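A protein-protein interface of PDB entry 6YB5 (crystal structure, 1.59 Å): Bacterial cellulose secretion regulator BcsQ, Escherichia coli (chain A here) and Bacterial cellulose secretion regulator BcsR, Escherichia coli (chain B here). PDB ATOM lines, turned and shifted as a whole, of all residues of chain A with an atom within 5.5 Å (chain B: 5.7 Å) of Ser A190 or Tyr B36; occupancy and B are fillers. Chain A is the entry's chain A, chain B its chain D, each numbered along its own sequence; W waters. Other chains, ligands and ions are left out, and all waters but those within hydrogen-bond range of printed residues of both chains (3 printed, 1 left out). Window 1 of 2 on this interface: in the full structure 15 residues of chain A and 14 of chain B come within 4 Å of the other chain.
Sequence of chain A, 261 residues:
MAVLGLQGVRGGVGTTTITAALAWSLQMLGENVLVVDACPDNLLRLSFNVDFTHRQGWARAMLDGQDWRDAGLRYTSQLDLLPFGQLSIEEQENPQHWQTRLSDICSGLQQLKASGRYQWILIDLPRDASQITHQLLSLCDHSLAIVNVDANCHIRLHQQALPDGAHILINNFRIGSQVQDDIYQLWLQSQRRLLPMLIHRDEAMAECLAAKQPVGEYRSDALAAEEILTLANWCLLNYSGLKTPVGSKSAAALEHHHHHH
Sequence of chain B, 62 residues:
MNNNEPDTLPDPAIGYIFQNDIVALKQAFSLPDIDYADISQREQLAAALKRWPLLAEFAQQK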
ATOM      1  N   HIS A 154     -14.582  17.135  28.054  1.00  0.00           N
ATOM      2  CA  HIS A 154     -15.422  16.266  27.226  1.00  0.00           C
ATOM      3  C   HIS A 154     -14.673  15.804  25.981  1.00  0.00           C
ATOM      4  O   HIS A 154     -14.635  14.608  25.664  1.00  0.00           O
ATOM      5  CB  HIS A 154     -16.704  16.998  26.835  1.00  0.00           C
ATOM      6  CG  HIS A 154     -17.646  16.168  26.022  1.00  0.00           C
ATOM      7  ND1 HIS A 154     -18.419  15.169  26.575  1.00  0.00           N
ATOM      8  CD2 HIS A 154     -17.947  16.193  24.701  1.00  0.00           C
ATOM      9  CE1 HIS A 154     -19.164  14.620  25.630  1.00  0.00           C
ATOM     10  NE2 HIS A 154     -18.890  15.215  24.482  1.00  0.00           N
ATOM     11  N   HIS A 158     -12.478  11.722  24.653  1.00  0.00           N
ATOM     12  CA  HIS A 158     -12.638  11.035  23.375  1.00  0.00           C
ATOM     13  C   HIS A 158     -11.338  10.885  22.591  1.00  0.00           C
ATOM     14  O   HIS A 158     -11.355  10.286  21.509  1.00  0.00           O
ATOM     15  CB  HIS A 158     -13.653  11.778  22.494  1.00  0.00           C
ATOM     16  CG  HIS A 158     -15.047  11.784  23.037  1.00  0.00           C
ATOM     17  ND1 HIS A 158     -15.470  12.669  24.010  1.00  0.00           N
ATOM     18  CD2 HIS A 158     -16.120  11.016  22.732  1.00  0.00           C
ATOM     19  CE1 HIS A 158     -16.744  12.440  24.283  1.00  0.00           C
ATOM     20  NE2 HIS A 158     -17.161  11.440  23.523  1.00  0.00           N
ATOM     21  N   LEU A 186     -25.363  13.952  29.748  1.00  0.00           N
ATOM     22  CA  LEU A 186     -24.858  13.087  28.687  1.00  0.00           C
ATOM     23  C   LEU A 186     -23.845  12.085  29.228  1.00  0.00           C
ATOM     24  O   LEU A 186     -23.874  10.905  28.857  1.00  0.00           O
ATOM     25  CB  LEU A 186     -24.236  13.943  27.576  1.00  0.00           C
ATOM     26  CG  LEU A 186     -23.655  13.192  26.377  1.00  0.00           C
ATOM     27  CD1 LEU A 186     -24.711  12.301  25.719  1.00  0.00           C
ATOM     28  CD2 LEU A 186     -23.086  14.189  25.381  1.00  0.00           C
ATOM     29  N   TRP A 187     -22.932  12.539  30.097  1.00  0.00           N
ATOM     30  CA  TRP A 187     -21.956  11.629  30.703  1.00  0.00           C
ATOM     31  C   TRP A 187     -22.633  10.534  31.516  1.00  0.00           C
ATOM     32  O   TRP A 187     -22.191   9.378  31.503  1.00  0.00           O
ATOM     33  CB  TRP A 187     -20.992  12.399  31.605  1.00  0.00           C
ATOM     34  CG  TRP A 187     -19.958  13.205  30.892  1.00  0.00           C
ATOM     35  CD1 TRP A 187     -19.857  13.427  29.546  1.00  0.00           C
ATOM     36  CD2 TRP A 187     -18.871  13.901  31.503  1.00  0.00           C
ATOM     37  NE1 TRP A 187     -18.768  14.233  29.284  1.00  0.00           N
ATOM     38  CE2 TRP A 187     -18.146  14.534  30.471  1.00  0.00           C
ATOM     39  CE3 TRP A 187     -18.438  14.047  32.828  1.00  0.00           C
ATOM     40  CZ2 TRP A 187     -17.012  15.307  30.725  1.00  0.00           C
ATOM     41  CZ3 TRP A 187     -17.317  14.815  33.078  1.00  0.00           C
ATOM     42  CH2 TRP A 187     -16.626  15.445  32.036  1.00  0.00           C
ATOM     43  N   LEU A 188     -23.696  10.878  32.252  1.00  0.00           N
ATOM     44  CA  LEU A 188     -24.363   9.872  33.076  1.00  0.00           C
ATOM     45  C   LEU A 188     -24.875   8.714  32.235  1.00  0.00           C
ATOM     46  O   LEU A 188     -24.923   7.574  32.713  1.00  0.00           O
ATOM     47  CB  LEU A 188     -25.517  10.499  33.857  1.00  0.00           C
ATOM     48  CG  LEU A 188     -25.099  11.442  34.986  1.00  0.00           C
ATOM     49  CD1 LEU A 188     -26.319  12.150  35.520  1.00  0.00           C
ATOM     50  CD2 LEU A 188     -24.401  10.686  36.094  1.00  0.00           C
ATOM     51  N   GLN A 189     -25.235   8.981  30.981  1.00  0.00           N
ATOM     52  CA  GLN A 189     -25.782   7.976  30.077  1.00  0.00           C
ATOM     53  C   GLN A 189     -24.732   7.296  29.208  1.00  0.00           C
ATOM     54  O   GLN A 189     -25.063   6.313  28.535  1.00  0.00           O
ATOM     55  CB  GLN A 189     -26.820   8.611  29.144  1.00  0.00           C
ATOM     56  CG  GLN A 189     -28.043   9.160  29.847  1.00  0.00           C
ATOM     57  CD  GLN A 189     -28.909   8.066  30.414  1.00  0.00           C
ATOM     58  OE1 GLN A 189     -29.334   7.162  29.693  1.00  0.00           O
ATOM     59  NE2 GLN A 189     -29.165   8.129  31.715  1.00  0.00           N
ATOM     60  N   SER A 190     -23.498   7.792  29.175  1.00  0.00           N
ATOM     61  CA  SER A 190     -22.524   7.303  28.209  1.00  0.00           C
ATOM     62  C   SER A 190     -21.135   7.003  28.774  1.00  0.00           C
ATOM     63  O   SER A 190     -20.418   6.201  28.163  1.00  0.00           O
ATOM     64  CB  SER A 190     -22.380   8.310  27.052  1.00  0.00           C
ATOM     65  OG  SER A 190     -21.913   9.566  27.538  1.00  0.00           O
ATOM     66  N   GLN A 191     -20.723   7.606  29.895  1.00  0.00           N
ATOM     67  CA  GLN A 191     -19.363   7.430  30.415  1.00  0.00           C
ATOM     68  C   GLN A 191     -19.363   6.301  31.444  1.00  0.00           C
ATOM     69  O   GLN A 191     -19.699   6.501  32.613  1.00  0.00           O
ATOM     70  CB  GLN A 191     -18.840   8.729  31.019  1.00  0.00           C
ATOM     71  CG  GLN A 191     -18.707   9.860  29.997  1.00  0.00           C
ATOM     72  CD  GLN A 191     -17.424   9.780  29.171  1.00  0.00           C
ATOM     73  OE1 GLN A 191     -16.453   9.132  29.571  1.00  0.00           O
ATOM     74  NE2 GLN A 191     -17.419  10.435  28.002  1.00  0.00           N
ATOM     75  N   ARG A 192     -18.958   5.110  31.019  1.00  0.00           N
ATOM     76  CA  ARG A 192     -19.062   3.952  31.900  1.00  0.00           C
ATOM     77  C   ARG A 192     -18.083   3.993  33.068  1.00  0.00           C
ATOM     78  O   ARG A 192     -18.255   3.232  34.025  1.00  0.00           O
ATOM     79  CB  ARG A 192     -18.865   2.676  31.080  1.00  0.00           C
ATOM     80  CG  ARG A 192     -19.950   2.487  30.025  1.00  0.00           C
ATOM     81  CD  ARG A 192     -19.634   1.332  29.082  1.00  0.00           C
ATOM     82  NE  ARG A 192     -19.452   0.064  29.784  1.00  0.00           N
ATOM     83  CZ  ARG A 192     -18.270  -0.507  30.008  1.00  0.00           C
ATOM     84  NH1 ARG A 192     -17.156   0.074  29.581  1.00  0.00           N
ATOM     85  NH2 ARG A 192     -18.203  -1.665  30.657  1.00  0.00           N
ATOM     86  N   ASP B  33     -15.359   2.443  26.643  1.00  0.00           N
ATOM     87  CA  ASP B  33     -15.529   3.252  27.845  1.00  0.00           C
ATOM     88  C   ASP B  33     -16.597   4.318  27.666  1.00  0.00           C
ATOM     89  O   ASP B  33     -17.152   4.797  28.663  1.00  0.00           O
ATOM     90  CB  ASP B  33     -14.212   3.930  28.220  1.00  0.00           C
ATOM     91  CG  ASP B  33     -13.162   2.947  28.703  1.00  0.00           C
ATOM     92  OD1 ASP B  33     -13.526   1.968  29.390  1.00  0.00           O
ATOM     93  OD2 ASP B  33     -11.971   3.164  28.398  1.00  0.00           O
ATOM     94  N   ILE B  34     -16.869   4.715  26.426  1.00  0.00           N
ATOM     95  CA  ILE B  34     -17.907   5.686  26.102  1.00  0.00           C
ATOM     96  C   ILE B  34     -18.879   4.997  25.165  1.00  0.00           C
ATOM     97  O   ILE B  34     -18.478   4.482  24.113  1.00  0.00           O
ATOM     98  CB  ILE B  34     -17.333   6.961  25.461  1.00  0.00           C
ATOM     99  CG1 ILE B  34     -16.200   7.525  26.310  1.00  0.00           C
ATOM    100  CG2 ILE B  34     -18.441   7.998  25.274  1.00  0.00           C
ATOM    101  CD1 ILE B  34     -15.494   8.718  25.660  1.00  0.00           C
ATOM    102  N   ASP B  35     -20.150   4.976  25.541  1.00  0.00           N
ATOM    103  CA  ASP B  35     -21.149   4.171  24.847  1.00  0.00           C
ATOM    104  C   ASP B  35     -22.342   5.064  24.539  1.00  0.00           C
ATOM    105  O   ASP B  35     -23.099   5.422  25.446  1.00  0.00           O
ATOM    106  CB  ASP B  35     -21.550   2.965  25.706  1.00  0.00           C
ATOM    107  CG  ASP B  35     -22.574   2.067  25.031  1.00  0.00           C
ATOM    108  OD1 ASP B  35     -22.903   2.285  23.850  1.00  0.00           O
ATOM    109  OD2 ASP B  35     -23.060   1.129  25.702  1.00  0.00           O
ATOM    110  N   TYR B  36     -22.516   5.421  23.264  1.00  0.00           N
ATOM    111  CA  TYR B  36     -23.625   6.267  22.840  1.00  0.00           C
ATOM    112  C   TYR B  36     -24.822   5.476  22.314  1.00  0.00           C
ATOM    113  O   TYR B  36     -25.704   6.056  21.673  1.00  0.00           O
ATOM    114  CB  TYR B  36     -23.153   7.264  21.782  1.00  0.00           C
ATOM    115  CG  TYR B  36     -22.259   8.351  22.328  1.00  0.00           C
ATOM    116  CD1 TYR B  36     -22.756   9.298  23.221  1.00  0.00           C
ATOM    117  CD2 TYR B  36     -20.925   8.445  21.947  1.00  0.00           C
ATOM    118  CE1 TYR B  36     -21.948  10.306  23.718  1.00  0.00           C
ATOM    119  CE2 TYR B  36     -20.104   9.452  22.442  1.00  0.00           C
ATOM    120  CZ  TYR B  36     -20.621  10.375  23.327  1.00  0.00           C
ATOM    121  OH  TYR B  36     -19.805  11.366  23.811  1.00  0.00           O
ATOM    122  N   ALA B  37     -24.898   4.176  22.595  1.00  0.00           N
ATOM    123  CA  ALA B  37     -26.013   3.383  22.092  1.00  0.00           C
ATOM    124  C   ALA B  37     -27.333   3.891  22.662  1.00  0.00           C
ATOM    125  O   ALA B  37     -27.462   4.091  23.872  1.00  0.00           O
ATOM    126  CB  ALA B  37     -25.820   1.910  22.444  1.00  0.00           C
ATOM    127  N   ASP B  38     -28.302   4.122  21.779  1.00  0.00           N
ATOM    128  CA  ASP B  38     -29.647   4.578  22.137  1.00  0.00           C
ATOM    129  C   ASP B  38     -29.656   5.969  22.772  1.00  0.00           C
ATOM    130  O   ASP B  38     -30.614   6.323  23.469  1.00  0.00           O
ATOM    131  CB  ASP B  38     -30.346   3.580  23.068  1.00  0.00           C
ATOM    132  CG  ASP B  38     -30.181   2.144  22.614  1.00  0.00           C
ATOM    133  OD1 ASP B  38     -30.095   1.911  21.391  1.00  0.00           O
ATOM    134  OD2 ASP B  38     -30.132   1.248  23.485  1.00  0.00           O
ATOM    135  N   ILE B  39     -28.611   6.770  22.549  1.00  0.00           N
ATOM    136  CA  ILE B  39     -28.572   8.112  23.126  1.00  0.00           C
ATOM    137  C   ILE B  39     -29.660   8.993  22.523  1.00  0.00           C
ATOM    138  O   ILE B  39     -30.283   9.801  23.221  1.00  0.00           O
ATOM    139  CB  ILE B  39     -27.173   8.729  22.950  1.00  0.00           C
ATOM    140  CG1 ILE B  39     -26.266   8.312  24.106  1.00  0.00           C
ATOM    141  CG2 ILE B  39     -27.245  10.246  22.848  1.00  0.00           C
ATOM    142  CD1 ILE B  39     -26.740   8.787  25.443  1.00  0.00           C
ATOM    143  N   SER B  40     -29.920   8.843  21.226  1.00  0.00           N
ATOM    144  CA  SER B  40     -30.920   9.653  20.542  1.00  0.00           C
ATOM    145  C   SER B  40     -32.349   9.204  20.831  1.00  0.00           C
ATOM    146  O   SER B  40     -33.274   9.637  20.136  1.00  0.00           O
ATOM    147  CB  SER B  40     -30.660   9.644  19.034  1.00  0.00           C
ATOM    148  OG  SER B  40     -29.441  10.303  18.728  1.00  0.00           O
ATOM    149  N   LEU B  55     -21.400  18.448  21.295  1.00  0.00           N
ATOM    150  CA  LEU B  55     -21.894  17.211  21.905  1.00  0.00           C
ATOM    151  C   LEU B  55     -22.534  16.310  20.860  1.00  0.00           C
ATOM    152  O   LEU B  55     -22.397  15.077  20.915  1.00  0.00           O
ATOM    153  CB  LEU B  55     -22.903  17.534  23.009  1.00  0.00           C
ATOM    154  CG  LEU B  55     -22.421  18.440  24.145  1.00  0.00           C
ATOM    155  CD1 LEU B  55     -23.460  18.483  25.274  1.00  0.00           C
ATOM    156  CD2 LEU B  55     -21.065  17.984  24.672  1.00  0.00           C
ATOM    157  N   PHE B  58     -20.003  14.014  18.650  1.00  0.00           N
ATOM    158  CA  PHE B  58     -19.484  12.782  19.236  1.00  0.00           C
ATOM    159  C   PHE B  58     -20.558  11.711  19.352  1.00  0.00           C
ATOM    160  O   PHE B  58     -20.251  10.518  19.244  1.00  0.00           O
ATOM    161  CB  PHE B  58     -18.896  13.043  20.624  1.00  0.00           C
ATOM    162  CG  PHE B  58     -17.639  13.858  20.608  1.00  0.00           C
ATOM    163  CD1 PHE B  58     -16.437  13.287  20.211  1.00  0.00           C
ATOM    164  CD2 PHE B  58     -17.653  15.179  21.001  1.00  0.00           C
ATOM    165  CE1 PHE B  58     -15.263  14.044  20.203  1.00  0.00           C
ATOM    166  CE2 PHE B  58     -16.485  15.944  20.991  1.00  0.00           C
ATOM    167  CZ  PHE B  58     -15.292  15.369  20.591  1.00  0.00           C
ATOM    168  N   ALA B  59     -21.803  12.119  19.588  1.00  0.00           N
ATOM    169  CA  ALA B  59     -22.891  11.193  19.875  1.00  0.00           C
ATOM    170  C   ALA B  59     -23.570  10.660  18.622  1.00  0.00           C
ATOM    171  O   ALA B  59     -24.322   9.684  18.713  1.00  0.00           O
ATOM    172  CB  ALA B  59     -23.933  11.874  20.777  1.00  0.00           C
HETATM  173  O   HOH W   1     -16.059   6.472  30.604  1.00  0.00           O
HETATM  174  O   HOH W   2     -20.911  14.057  23.032  1.00  0.00           O
HETATM  175  O   HOH W   3     -19.974  11.353  26.637  1.00  0.00           O
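Printed residues of chain B that touch a printed residue of chain A: Asp B33, Ile B34, Asp B35, Tyr B36, Ile B39, Leu B55 and Phe B58. Among the printed residues, no Asp or Glu carboxylate lies within 4 Å of a Lys or Arg side-chain nitrogen of the other chain.
Water W2 lies within hydrogen-bond range of NE2 of His A154, O of Leu B55 and OH of Tyr B36. Water W3 lies within hydrogen-bond range of OG of Ser A190, OH of Tyr B36 and NE2 of Gln A191. Water W1 lies within hydrogen-bond range of O of Asp B33, OE1 of Gln A191 and N of Arg A192.
OH of Tyr B36 lies within hydrogen-bond range of NE2 of His A158 (2.7 Å). The backbone carbonyl oxygen (O) of Ser A190 is in hydrogen-bond range of the backbone NH (N) of Asp B35, 2.9 Å away. The backbone carbonyl oxygen (O) of Asp B33 is in hydrogen-bond range of the backbone NH (N) of Arg A192 (3.0 Å).
Trp A187 touches none of the printed residues of chain B. Leu A188 touches none of the printed residues of chain B. Ser A190 touches just these residues of chain B: Asp B33 (3.6 Å), Ile B34 (3.3 Å), Asp B35 (2.9 Å) and Tyr B36 (3.9 Å). Printed residues of chain B within 4 Å of Arg A192: Asp B33 (3.0 Å). Of the printed residues of chain A, Asp B33 touches Ser A190 (3.6 Å), Gln A191 (3.9 Å) and Arg A192 (3.0 Å). Of the printed residues of chain A, Tyr B36 touches His A154, His A158, Leu A186 and Ser A190. Printed residues of chain A within 4 Å of Leu B55: His A154. The nearest printed residue of chain A that does not touch Leu B55 is Leu A186 (4.1 Å).
His A154 touches Leu B55. His A154 touches Phe B58. His A158 touches Ile B34. CD2 of His A158 touches CD1 of Phe B58 (3.4 Å). Leu A186 touches Tyr B36. Asp B35 touches Gln A189. Gln A189 touches Ile B39. CA of Ile B34 touches O of Ser A190, 3.3 Å away. OG of Ser A190 touches CE1 of Tyr B36, at 3.9 Å. NE2 of Gln A191 touches CD1 of Ile B34, at 3.5 Å.
O of His A154 sits at hydrogen-bond distance from ND1 of His A158 (2.7 Å). ND1 of His A154 lies within hydrogen-bond range of NE1 of Trp A187, at 2.9 Å. OG of Ser A190 is in hydrogen-bond range of O of Leu A186, 2.7 Å away. The side-chain carboxylate (OD1) of Asp B35 lies within hydrogen-bond range of the backbone NH (N) of Ala B37 (3.0 Å).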
